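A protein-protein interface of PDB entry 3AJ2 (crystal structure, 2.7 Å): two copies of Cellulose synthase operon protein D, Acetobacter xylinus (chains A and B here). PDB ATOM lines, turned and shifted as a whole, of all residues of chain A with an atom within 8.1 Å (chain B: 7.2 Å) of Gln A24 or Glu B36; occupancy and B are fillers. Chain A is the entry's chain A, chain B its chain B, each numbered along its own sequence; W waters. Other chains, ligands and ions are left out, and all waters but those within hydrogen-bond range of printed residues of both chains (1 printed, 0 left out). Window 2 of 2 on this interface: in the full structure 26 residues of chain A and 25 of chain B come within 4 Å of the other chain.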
ATOM      1  N   THR A  16     -24.248 -15.492  36.117  1.00  0.00           N
ATOM      2  CA  THR A  16     -23.543 -14.818  35.036  1.00  0.00           C
ATOM      3  C   THR A  16     -24.399 -13.741  34.367  1.00  0.00           C
ATOM      4  O   THR A  16     -23.872 -12.675  33.969  1.00  0.00           O
ATOM      5  CB  THR A  16     -22.944 -15.847  34.034  1.00  0.00           C
ATOM      6  OG1 THR A  16     -23.926 -16.852  33.772  1.00  0.00           O
ATOM      7  CG2 THR A  16     -21.729 -16.552  34.666  1.00  0.00           C
ATOM      8  N   LEU A  17     -25.711 -14.000  34.297  1.00  0.00           N
ATOM      9  CA  LEU A  17     -26.675 -13.026  33.783  1.00  0.00           C
ATOM     10  C   LEU A  17     -26.753 -11.791  34.661  1.00  0.00           C
ATOM     11  O   LEU A  17     -26.600 -10.650  34.184  1.00  0.00           O
ATOM     12  CB  LEU A  17     -28.060 -13.632  33.601  1.00  0.00           C
ATOM     13  CG  LEU A  17     -29.166 -12.649  33.173  1.00  0.00           C
ATOM     14  CD1 LEU A  17     -29.007 -12.106  31.770  1.00  0.00           C
ATOM     15  CD2 LEU A  17     -30.484 -13.349  33.263  1.00  0.00           C
ATOM     16  N   SER A  18     -26.966 -11.998  35.949  1.00  0.00           N
ATOM     17  CA  SER A  18     -26.978 -10.862  36.852  1.00  0.00           C
ATOM     18  C   SER A  18     -25.718  -9.993  36.649  1.00  0.00           C
ATOM     19  O   SER A  18     -25.794  -8.776  36.445  1.00  0.00           O
ATOM     20  CB  SER A  18     -27.171 -11.314  38.305  1.00  0.00           C
ATOM     21  OG  SER A  18     -26.094 -12.093  38.812  1.00  0.00           O
ATOM     22  N   TRP A  19     -24.567 -10.635  36.643  1.00  0.00           N
ATOM     23  CA  TRP A  19     -23.320  -9.934  36.460  1.00  0.00           C
ATOM     24  C   TRP A  19     -23.330  -9.143  35.195  1.00  0.00           C
ATOM     25  O   TRP A  19     -23.000  -7.944  35.192  1.00  0.00           O
ATOM     26  CB  TRP A  19     -22.183 -10.930  36.397  1.00  0.00           C
ATOM     27  CG  TRP A  19     -21.380 -10.986  37.645  1.00  0.00           C
ATOM     28  CD1 TRP A  19     -21.755 -11.485  38.906  1.00  0.00           C
ATOM     29  CD2 TRP A  19     -20.049 -10.546  37.773  1.00  0.00           C
ATOM     30  NE1 TRP A  19     -20.696 -11.363  39.806  1.00  0.00           N
ATOM     31  CE2 TRP A  19     -19.640 -10.797  39.138  1.00  0.00           C
ATOM     32  CE3 TRP A  19     -19.152  -9.985  36.877  1.00  0.00           C
ATOM     33  CZ2 TRP A  19     -18.389 -10.474  39.610  1.00  0.00           C
ATOM     34  CZ3 TRP A  19     -17.901  -9.665  37.347  1.00  0.00           C
ATOM     35  CH2 TRP A  19     -17.522  -9.912  38.707  1.00  0.00           C
ATOM     36  N   GLU A  20     -23.704  -9.802  34.100  1.00  0.00           N
ATOM     37  CA  GLU A  20     -23.670  -9.093  32.839  1.00  0.00           C
ATOM     38  C   GLU A  20     -24.570  -7.857  32.875  1.00  0.00           C
ATOM     39  O   GLU A  20     -24.119  -6.733  32.610  1.00  0.00           O
ATOM     40  CB  GLU A  20     -24.006  -9.997  31.674  1.00  0.00           C
ATOM     41  CG  GLU A  20     -23.360  -9.520  30.392  1.00  0.00           C
ATOM     42  CD  GLU A  20     -21.839  -9.504  30.480  1.00  0.00           C
ATOM     43  OE1 GLU A  20     -21.247 -10.440  31.057  1.00  0.00           O
ATOM     44  OE2 GLU A  20     -21.222  -8.563  29.959  1.00  0.00           O
ATOM     45  N   ILE A  21     -25.829  -8.051  33.240  1.00  0.00           N
ATOM     46  CA  ILE A  21     -26.691  -6.899  33.352  1.00  0.00           C
ATOM     47  C   ILE A  21     -26.046  -5.801  34.243  1.00  0.00           C
ATOM     48  O   ILE A  21     -25.905  -4.672  33.784  1.00  0.00           O
ATOM     49  CB  ILE A  21     -28.100  -7.294  33.805  1.00  0.00           C
ATOM     50  CG1 ILE A  21     -28.808  -8.061  32.692  1.00  0.00           C
ATOM     51  CG2 ILE A  21     -28.927  -6.063  34.204  1.00  0.00           C
ATOM     52  CD1 ILE A  21     -29.973  -8.907  33.181  1.00  0.00           C
ATOM     53  N   ASP A  22     -25.652  -6.139  35.485  1.00  0.00           N
ATOM     54  CA  ASP A  22     -25.193  -5.144  36.492  1.00  0.00           C
ATOM     55  C   ASP A  22     -23.996  -4.342  36.029  1.00  0.00           C
ATOM     56  O   ASP A  22     -23.710  -3.231  36.522  1.00  0.00           O
ATOM     57  CB  ASP A  22     -24.843  -5.801  37.820  1.00  0.00           C
ATOM     58  CG  ASP A  22     -26.075  -6.173  38.637  1.00  0.00           C
ATOM     59  OD1 ASP A  22     -27.205  -6.155  38.081  1.00  0.00           O
ATOM     60  OD2 ASP A  22     -25.902  -6.485  39.841  1.00  0.00           O
ATOM     61  N   ASP A  23     -23.312  -4.927  35.060  1.00  0.00           N
ATOM     62  CA  ASP A  23     -22.152  -4.343  34.430  1.00  0.00           C
ATOM     63  C   ASP A  23     -22.557  -3.239  33.471  1.00  0.00           C
ATOM     64  O   ASP A  23     -21.980  -2.151  33.446  1.00  0.00           O
ATOM     65  CB  ASP A  23     -21.500  -5.449  33.621  1.00  0.00           C
ATOM     66  CG  ASP A  23     -20.059  -5.636  33.952  1.00  0.00           C
ATOM     67  OD1 ASP A  23     -19.640  -6.803  33.809  1.00  0.00           O
ATOM     68  OD2 ASP A  23     -19.354  -4.660  34.356  1.00  0.00           O
ATOM     69  N   GLN A  24     -23.574  -3.557  32.688  1.00  0.00           N
ATOM     70  CA  GLN A  24     -23.948  -2.794  31.560  1.00  0.00           C
ATOM     71  C   GLN A  24     -25.076  -1.842  31.846  1.00  0.00           C
ATOM     72  O   GLN A  24     -25.144  -0.833  31.208  1.00  0.00           O
ATOM     73  CB  GLN A  24     -24.343  -3.735  30.447  1.00  0.00           C
ATOM     74  CG  GLN A  24     -23.218  -4.629  29.966  1.00  0.00           C
ATOM     75  CD  GLN A  24     -23.647  -5.493  28.778  1.00  0.00           C
ATOM     76  OE1 GLN A  24     -24.453  -5.067  27.946  1.00  0.00           O
ATOM     77  NE2 GLN A  24     -23.100  -6.711  28.688  1.00  0.00           N
ATOM     78  N   VAL A  25     -25.956  -2.100  32.806  1.00  0.00           N
ATOM     79  CA  VAL A  25     -27.151  -1.233  32.866  1.00  0.00           C
ATOM     80  C   VAL A  25     -27.351  -0.310  34.075  1.00  0.00           C
ATOM     81  O   VAL A  25     -27.965   0.767  34.002  1.00  0.00           O
ATOM     82  CB  VAL A  25     -28.445  -1.992  32.482  1.00  0.00           C
ATOM     83  CG1 VAL A  25     -28.157  -2.955  31.317  1.00  0.00           C
ATOM     84  CG2 VAL A  25     -29.015  -2.720  33.661  1.00  0.00           C
ATOM     85  N   GLY A  26     -26.812  -0.695  35.203  1.00  0.00           N
ATOM     86  CA  GLY A  26     -26.995   0.158  36.349  1.00  0.00           C
ATOM     87  C   GLY A  26     -27.639  -0.732  37.366  1.00  0.00           C
ATOM     88  O   GLY A  26     -27.700  -1.983  37.193  1.00  0.00           O
ATOM     89  N   ILE A  27     -28.080  -0.109  38.453  1.00  0.00           N
ATOM     90  CA  ILE A  27     -28.818  -0.863  39.412  1.00  0.00           C
ATOM     91  C   ILE A  27     -30.291  -0.454  39.363  1.00  0.00           C
ATOM     92  O   ILE A  27     -31.170  -1.311  39.446  1.00  0.00           O
ATOM     93  CB  ILE A  27     -28.180  -0.878  40.820  1.00  0.00           C
ATOM     94  CG1 ILE A  27     -28.879   0.065  41.744  1.00  0.00           C
ATOM     95  CG2 ILE A  27     -26.708  -0.618  40.780  1.00  0.00           C
ATOM     96  CD1 ILE A  27     -29.034  -0.546  43.058  1.00  0.00           C
ATOM     97  N   VAL A  29     -32.083   0.594  37.006  1.00  0.00           N
ATOM     98  CA  VAL A  29     -32.701   0.126  35.747  1.00  0.00           C
ATOM     99  C   VAL A  29     -32.909  -1.377  35.773  1.00  0.00           C
ATOM    100  O   VAL A  29     -33.937  -1.864  35.308  1.00  0.00           O
ATOM    101  CB  VAL A  29     -31.874   0.596  34.498  1.00  0.00           C
ATOM    102  CG1 VAL A  29     -32.037  -0.323  33.278  1.00  0.00           C
ATOM    103  CG2 VAL A  29     -32.220   2.056  34.172  1.00  0.00           C
ATOM    104  N   VAL B  29     -30.185  -7.176  19.957  1.00  0.00           N
ATOM    105  CA  VAL B  29     -29.580  -6.739  21.203  1.00  0.00           C
ATOM    106  C   VAL B  29     -29.715  -7.838  22.225  1.00  0.00           C
ATOM    107  O   VAL B  29     -28.774  -8.139  22.967  1.00  0.00           O
ATOM    108  CB  VAL B  29     -30.204  -5.454  21.726  1.00  0.00           C
ATOM    109  CG1 VAL B  29     -29.766  -5.210  23.138  1.00  0.00           C
ATOM    110  CG2 VAL B  29     -29.831  -4.269  20.814  1.00  0.00           C
ATOM    111  N   ARG B  30     -30.879  -8.463  22.267  1.00  0.00           N
ATOM    112  CA  ARG B  30     -31.036  -9.593  23.158  1.00  0.00           C
ATOM    113  C   ARG B  30     -29.994 -10.693  22.870  1.00  0.00           C
ATOM    114  O   ARG B  30     -29.241 -11.032  23.777  1.00  0.00           O
ATOM    115  CB  ARG B  30     -32.444 -10.144  23.108  1.00  0.00           C
ATOM    116  CG  ARG B  30     -32.583 -11.469  23.803  1.00  0.00           C
ATOM    117  CD  ARG B  30     -33.778 -12.152  23.280  1.00  0.00           C
ATOM    118  NE  ARG B  30     -33.438 -12.809  22.051  1.00  0.00           N
ATOM    119  CZ  ARG B  30     -34.304 -13.199  21.128  1.00  0.00           C
ATOM    120  NH1 ARG B  30     -35.597 -12.960  21.250  1.00  0.00           N
ATOM    121  NH2 ARG B  30     -33.843 -13.804  20.049  1.00  0.00           N
ATOM    122  N   ASN B  31     -29.922 -11.225  21.640  1.00  0.00           N
ATOM    123  CA  ASN B  31     -28.877 -12.220  21.299  1.00  0.00           C
ATOM    124  C   ASN B  31     -27.455 -11.812  21.750  1.00  0.00           C
ATOM    125  O   ASN B  31     -26.745 -12.609  22.390  1.00  0.00           O
ATOM    126  CB  ASN B  31     -28.847 -12.552  19.801  1.00  0.00           C
ATOM    127  CG  ASN B  31     -30.126 -13.199  19.303  1.00  0.00           C
ATOM    128  OD1 ASN B  31     -30.876 -13.835  20.041  1.00  0.00           O
ATOM    129  ND2 ASN B  31     -30.378 -13.035  18.019  1.00  0.00           N
ATOM    130  N   GLU B  32     -27.036 -10.584  21.416  1.00  0.00           N
ATOM    131  CA  GLU B  32     -25.711 -10.130  21.813  1.00  0.00           C
ATOM    132  C   GLU B  32     -25.535 -10.153  23.344  1.00  0.00           C
ATOM    133  O   GLU B  32     -24.562 -10.726  23.831  1.00  0.00           O
ATOM    134  CB  GLU B  32     -25.338  -8.780  21.181  1.00  0.00           C
ATOM    135  CG  GLU B  32     -23.794  -8.478  21.176  1.00  0.00           C
ATOM    136  CD  GLU B  32     -22.846  -9.731  20.920  1.00  0.00           C
ATOM    137  OE1 GLU B  32     -22.964 -10.441  19.872  1.00  0.00           O
ATOM    138  OE2 GLU B  32     -21.959  -9.984  21.772  1.00  0.00           O
ATOM    139  N   LEU B  33     -26.489  -9.578  24.084  1.00  0.00           N
ATOM    140  CA  LEU B  33     -26.562  -9.757  25.541  1.00  0.00           C
ATOM    141  C   LEU B  33     -26.357 -11.197  26.005  1.00  0.00           C
ATOM    142  O   LEU B  33     -25.553 -11.453  26.880  1.00  0.00           O
ATOM    143  CB  LEU B  33     -27.905  -9.250  26.102  1.00  0.00           C
ATOM    144  CG  LEU B  33     -28.151  -9.458  27.617  1.00  0.00           C
ATOM    145  CD1 LEU B  33     -26.985  -8.920  28.541  1.00  0.00           C
ATOM    146  CD2 LEU B  33     -29.508  -8.898  28.039  1.00  0.00           C
ATOM    147  N   LEU B  34     -27.087 -12.120  25.396  1.00  0.00           N
ATOM    148  CA  LEU B  34     -27.050 -13.529  25.756  1.00  0.00           C
ATOM    149  C   LEU B  34     -25.749 -14.238  25.383  1.00  0.00           C
ATOM    150  O   LEU B  34     -25.356 -15.187  26.060  1.00  0.00           O
ATOM    151  CB  LEU B  34     -28.232 -14.244  25.125  1.00  0.00           C
ATOM    152  CG  LEU B  34     -29.480 -14.720  25.901  1.00  0.00           C
ATOM    153  CD1 LEU B  34     -29.690 -14.172  27.319  1.00  0.00           C
ATOM    154  CD2 LEU B  34     -30.745 -14.568  24.990  1.00  0.00           C
ATOM    155  N   ARG B  35     -25.069 -13.785  24.331  1.00  0.00           N
ATOM    156  CA  ARG B  35     -23.752 -14.356  24.000  1.00  0.00           C
ATOM    157  C   ARG B  35     -22.706 -14.017  25.059  1.00  0.00           C
ATOM    158  O   ARG B  35     -21.921 -14.885  25.499  1.00  0.00           O
ATOM    159  CB  ARG B  35     -23.268 -13.880  22.648  1.00  0.00           C
ATOM    160  CG  ARG B  35     -23.834 -14.662  21.519  1.00  0.00           C
ATOM    161  CD  ARG B  35     -23.461 -14.070  20.174  1.00  0.00           C
ATOM    162  NE  ARG B  35     -24.523 -14.399  19.236  1.00  0.00           N
ATOM    163  CZ  ARG B  35     -25.299 -13.510  18.614  1.00  0.00           C
ATOM    164  NH1 ARG B  35     -25.097 -12.184  18.771  1.00  0.00           N
ATOM    165  NH2 ARG B  35     -26.260 -13.966  17.802  1.00  0.00           N
ATOM    166  N   GLU B  36     -22.709 -12.748  25.464  1.00  0.00           N
ATOM    167  CA  GLU B  36     -21.851 -12.269  26.531  1.00  0.00           C
ATOM    168  C   GLU B  36     -22.019 -13.053  27.840  1.00  0.00           C
ATOM    169  O   GLU B  36     -21.002 -13.460  28.446  1.00  0.00           O
ATOM    170  CB  GLU B  36     -22.095 -10.788  26.762  1.00  0.00           C
ATOM    171  CG  GLU B  36     -21.314  -9.905  25.853  1.00  0.00           C
ATOM    172  CD  GLU B  36     -22.000  -8.569  25.642  1.00  0.00           C
ATOM    173  OE1 GLU B  36     -23.107  -8.361  26.206  1.00  0.00           O
ATOM    174  OE2 GLU B  36     -21.439  -7.718  24.897  1.00  0.00           O
ATOM    175  N   VAL B  37     -23.272 -13.271  28.280  1.00  0.00           N
ATOM    176  CA  VAL B  37     -23.482 -14.095  29.485  1.00  0.00           C
ATOM    177  C   VAL B  37     -22.982 -15.504  29.226  1.00  0.00           C
ATOM    178  O   VAL B  37     -22.329 -16.112  30.091  1.00  0.00           O
ATOM    179  CB  VAL B  37     -24.937 -14.082  30.077  1.00  0.00           C
ATOM    180  CG1 VAL B  37     -25.897 -13.454  29.149  1.00  0.00           C
ATOM    181  CG2 VAL B  37     -25.421 -15.482  30.421  1.00  0.00           C
ATOM    182  N   GLY B  38     -23.252 -15.990  28.011  1.00  0.00           N
ATOM    183  CA  GLY B  38     -22.757 -17.283  27.564  1.00  0.00           C
ATOM    184  C   GLY B  38     -21.257 -17.396  27.717  1.00  0.00           C
ATOM    185  O   GLY B  38     -20.746 -18.405  28.212  1.00  0.00           O
ATOM    186  N   ARG B  39     -20.539 -16.358  27.300  1.00  0.00           N
ATOM    187  CA  ARG B  39     -19.087 -16.362  27.407  1.00  0.00           C
ATOM    188  C   ARG B  39     -18.643 -16.156  28.863  1.00  0.00           C
ATOM    189  O   ARG B  39     -17.606 -16.684  29.286  1.00  0.00           O
ATOM    190  CB  ARG B  39     -18.515 -15.350  26.419  1.00  0.00           C
ATOM    191  CG  ARG B  39     -17.231 -14.651  26.762  1.00  0.00           C
ATOM    192  CD  ARG B  39     -16.990 -13.611  25.680  1.00  0.00           C
ATOM    193  NE  ARG B  39     -16.235 -12.449  26.160  1.00  0.00           N
ATOM    194  CZ  ARG B  39     -14.932 -12.259  25.945  1.00  0.00           C
ATOM    195  NH1 ARG B  39     -14.233 -13.162  25.262  1.00  0.00           N
ATOM    196  NH2 ARG B  39     -14.322 -11.169  26.417  1.00  0.00           N
ATOM    197  N   GLY B  40     -19.444 -15.437  29.647  1.00  0.00           N
ATOM    198  CA  GLY B  40     -19.207 -15.378  31.092  1.00  0.00           C
ATOM    199  C   GLY B  40     -19.334 -16.727  31.805  1.00  0.00           C
ATOM    200  O   GLY B  40     -18.551 -17.029  32.710  1.00  0.00           O
ATOM    201  N   MET B  41     -20.330 -17.529  31.411  1.00  0.00           N
ATOM    202  CA  MET B  41     -20.482 -18.888  31.936  1.00  0.00           C
ATOM    203  C   MET B  41     -19.229 -19.682  31.637  1.00  0.00           C
ATOM    204  O   MET B  41     -18.789 -20.500  32.445  1.00  0.00           O
ATOM    205  CB  MET B  41     -21.666 -19.607  31.300  1.00  0.00           C
ATOM    206  CG  MET B  41     -22.958 -19.381  32.023  1.00  0.00           C
ATOM    207  SD  MET B  41     -24.456 -19.815  31.126  1.00  0.00           S
ATOM    208  CE  MET B  41     -24.595 -21.529  31.675  1.00  0.00           C
ATOM    209  N   GLY B  42     -18.643 -19.433  30.472  1.00  0.00           N
ATOM    210  CA  GLY B  42     -17.414 -20.110  30.124  1.00  0.00           C
ATOM    211  C   GLY B  42     -16.255 -19.702  31.000  1.00  0.00           C
ATOM    212  O   GLY B  42     -15.308 -20.447  31.081  1.00  0.00           O
ATOM    213  N   PRO B 106     -28.405 -18.312  21.888  1.00  0.00           N
ATOM    214  CA  PRO B 106     -27.192 -17.498  21.860  1.00  0.00           C
ATOM    215  C   PRO B 106     -26.277 -17.741  23.057  1.00  0.00           C
ATOM    216  O   PRO B 106     -25.074 -17.487  22.939  1.00  0.00           O
ATOM    217  CB  PRO B 106     -27.720 -16.063  21.901  1.00  0.00           C
ATOM    218  CG  PRO B 106     -29.129 -16.152  21.354  1.00  0.00           C
ATOM    219  CD  PRO B 106     -29.632 -17.491  21.824  1.00  0.00           C
ATOM    220  N   VAL B 107     -26.811 -18.219  24.191  1.00  0.00           N
ATOM    221  CA  VAL B 107     -25.954 -18.500  25.348  1.00  0.00           C
ATOM    222  C   VAL B 107     -24.993 -19.612  24.967  1.00  0.00           C
ATOM    223  O   VAL B 107     -23.786 -19.537  25.234  1.00  0.00           O
ATOM    224  CB  VAL B 107     -26.742 -18.880  26.609  1.00  0.00           C
ATOM    225  CG1 VAL B 107     -25.796 -19.152  27.794  1.00  0.00           C
ATOM    226  CG2 VAL B 107     -27.742 -17.784  26.963  1.00  0.00           C
ATOM    227  N   GLY B 110     -22.013 -18.376  22.911  1.00  0.00           N
ATOM    228  CA  GLY B 110     -21.009 -17.634  23.661  1.00  0.00           C
ATOM    229  C   GLY B 110     -20.249 -18.663  24.440  1.00  0.00           C
ATOM    230  O   GLY B 110     -19.034 -18.556  24.560  1.00  0.00           O
ATOM    231  N   LEU B 111     -20.972 -19.669  24.947  1.00  0.00           N
ATOM    232  CA  LEU B 111     -20.400 -20.694  25.801  1.00  0.00           C
ATOM    233  C   LEU B 111     -19.442 -21.590  25.008  1.00  0.00           C
ATOM    234  O   LEU B 111     -18.252 -21.675  25.347  1.00  0.00           O
ATOM    235  CB  LEU B 111     -21.506 -21.508  26.478  1.00  0.00           C
ATOM    236  CG  LEU B 111     -21.097 -22.666  27.405  1.00  0.00           C
ATOM    237  CD1 LEU B 111     -20.335 -22.186  28.626  1.00  0.00           C
ATOM    238  CD2 LEU B 111     -22.318 -23.479  27.832  1.00  0.00           C
ATOM    239  N   ARG B 114     -16.234 -19.592  24.018  1.00  0.00           N
ATOM    240  CA  ARG B 114     -15.217 -19.531  25.048  1.00  0.00           C
ATOM    241  C   ARG B 114     -14.611 -20.893  25.197  1.00  0.00           C
ATOM    242  O   ARG B 114     -13.391 -21.041  25.215  1.00  0.00           O
ATOM    243  CB  ARG B 114     -15.827 -19.093  26.388  1.00  0.00           C
ATOM    244  CG  ARG B 114     -14.822 -18.978  27.535  1.00  0.00           C
ATOM    245  CD  ARG B 114     -13.857 -17.804  27.366  1.00  0.00           C
ATOM    246  NE  ARG B 114     -14.392 -16.558  27.927  1.00  0.00           N
ATOM    247  CZ  ARG B 114     -13.924 -15.329  27.659  1.00  0.00           C
ATOM    248  NH1 ARG B 114     -12.903 -15.152  26.814  1.00  0.00           N
ATOM    249  NH2 ARG B 114     -14.485 -14.263  28.234  1.00  0.00           N
HETATM  250  O   HOH W   1     -24.705  -6.107  25.197  1.00  0.00           O
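Position printed for both chains: 29.
Of the 5 pairs that touch across the chains among the printed residues, none has its exchanged pair printed and touching as well.
NE2 of Gln A24 is in hydrogen-bond range of OE2 of Glu A20 (2.9 Å).
The side-chain carboxylate of Glu B36 sits at hydrogen-bond distance from the side-chain amide nitrogen of Gln A24.
Water W1 lies within hydrogen-bond range of the side-chain carboxylate of Glu B36 (2.9 Å) and the side-chain amide oxygen of Gln A24 (2.9 Å).
Hydrophobic or aromatic side chains of chain B that line the printed part of chain A: Val B37 and Met B41.
Of the 13 printed residues of chain A, 3 touch a printed residue of chain B.
Among the printed residues, 5 pairs touch across the chains.
Among the printed residues, no Asp or Glu carboxylate lies within 4 Å of a Lys or Arg side-chain nitrogen of the other chain.
Thr A16 touches Val B37.
Thr A16 touches Gly B40 (CG2 to C, 3.7 Å).
Met B41 touches Thr A16 (CG to OG1, 3.2 Å).
Glu A20 touches Glu B36.
Of chain B, only Glu B36 comes within 4 Å of Gln A24.
Of the printed residues of chain B, Thr A16 touches Val B37, Gly B40 and Met B41.
Of the printed residues of chain A, Met B41 touches Thr A16 (3.2 Å).
Of the printed residues of chain A, Gly B40 touches Thr A16 (3.7 Å).
Of the printed residues of chain B, Glu A20 touches Glu B36.
Gly A26 touches none of the printed residues of chain B.
Val A25 touches none of the printed residues of chain B.
The nearest residue of chain B that does not touch Gln A24 is Leu B33 (4.5 Å).
The nearest residue of chain A that does not touch Glu B36 is Thr A16 (6.3 Å).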
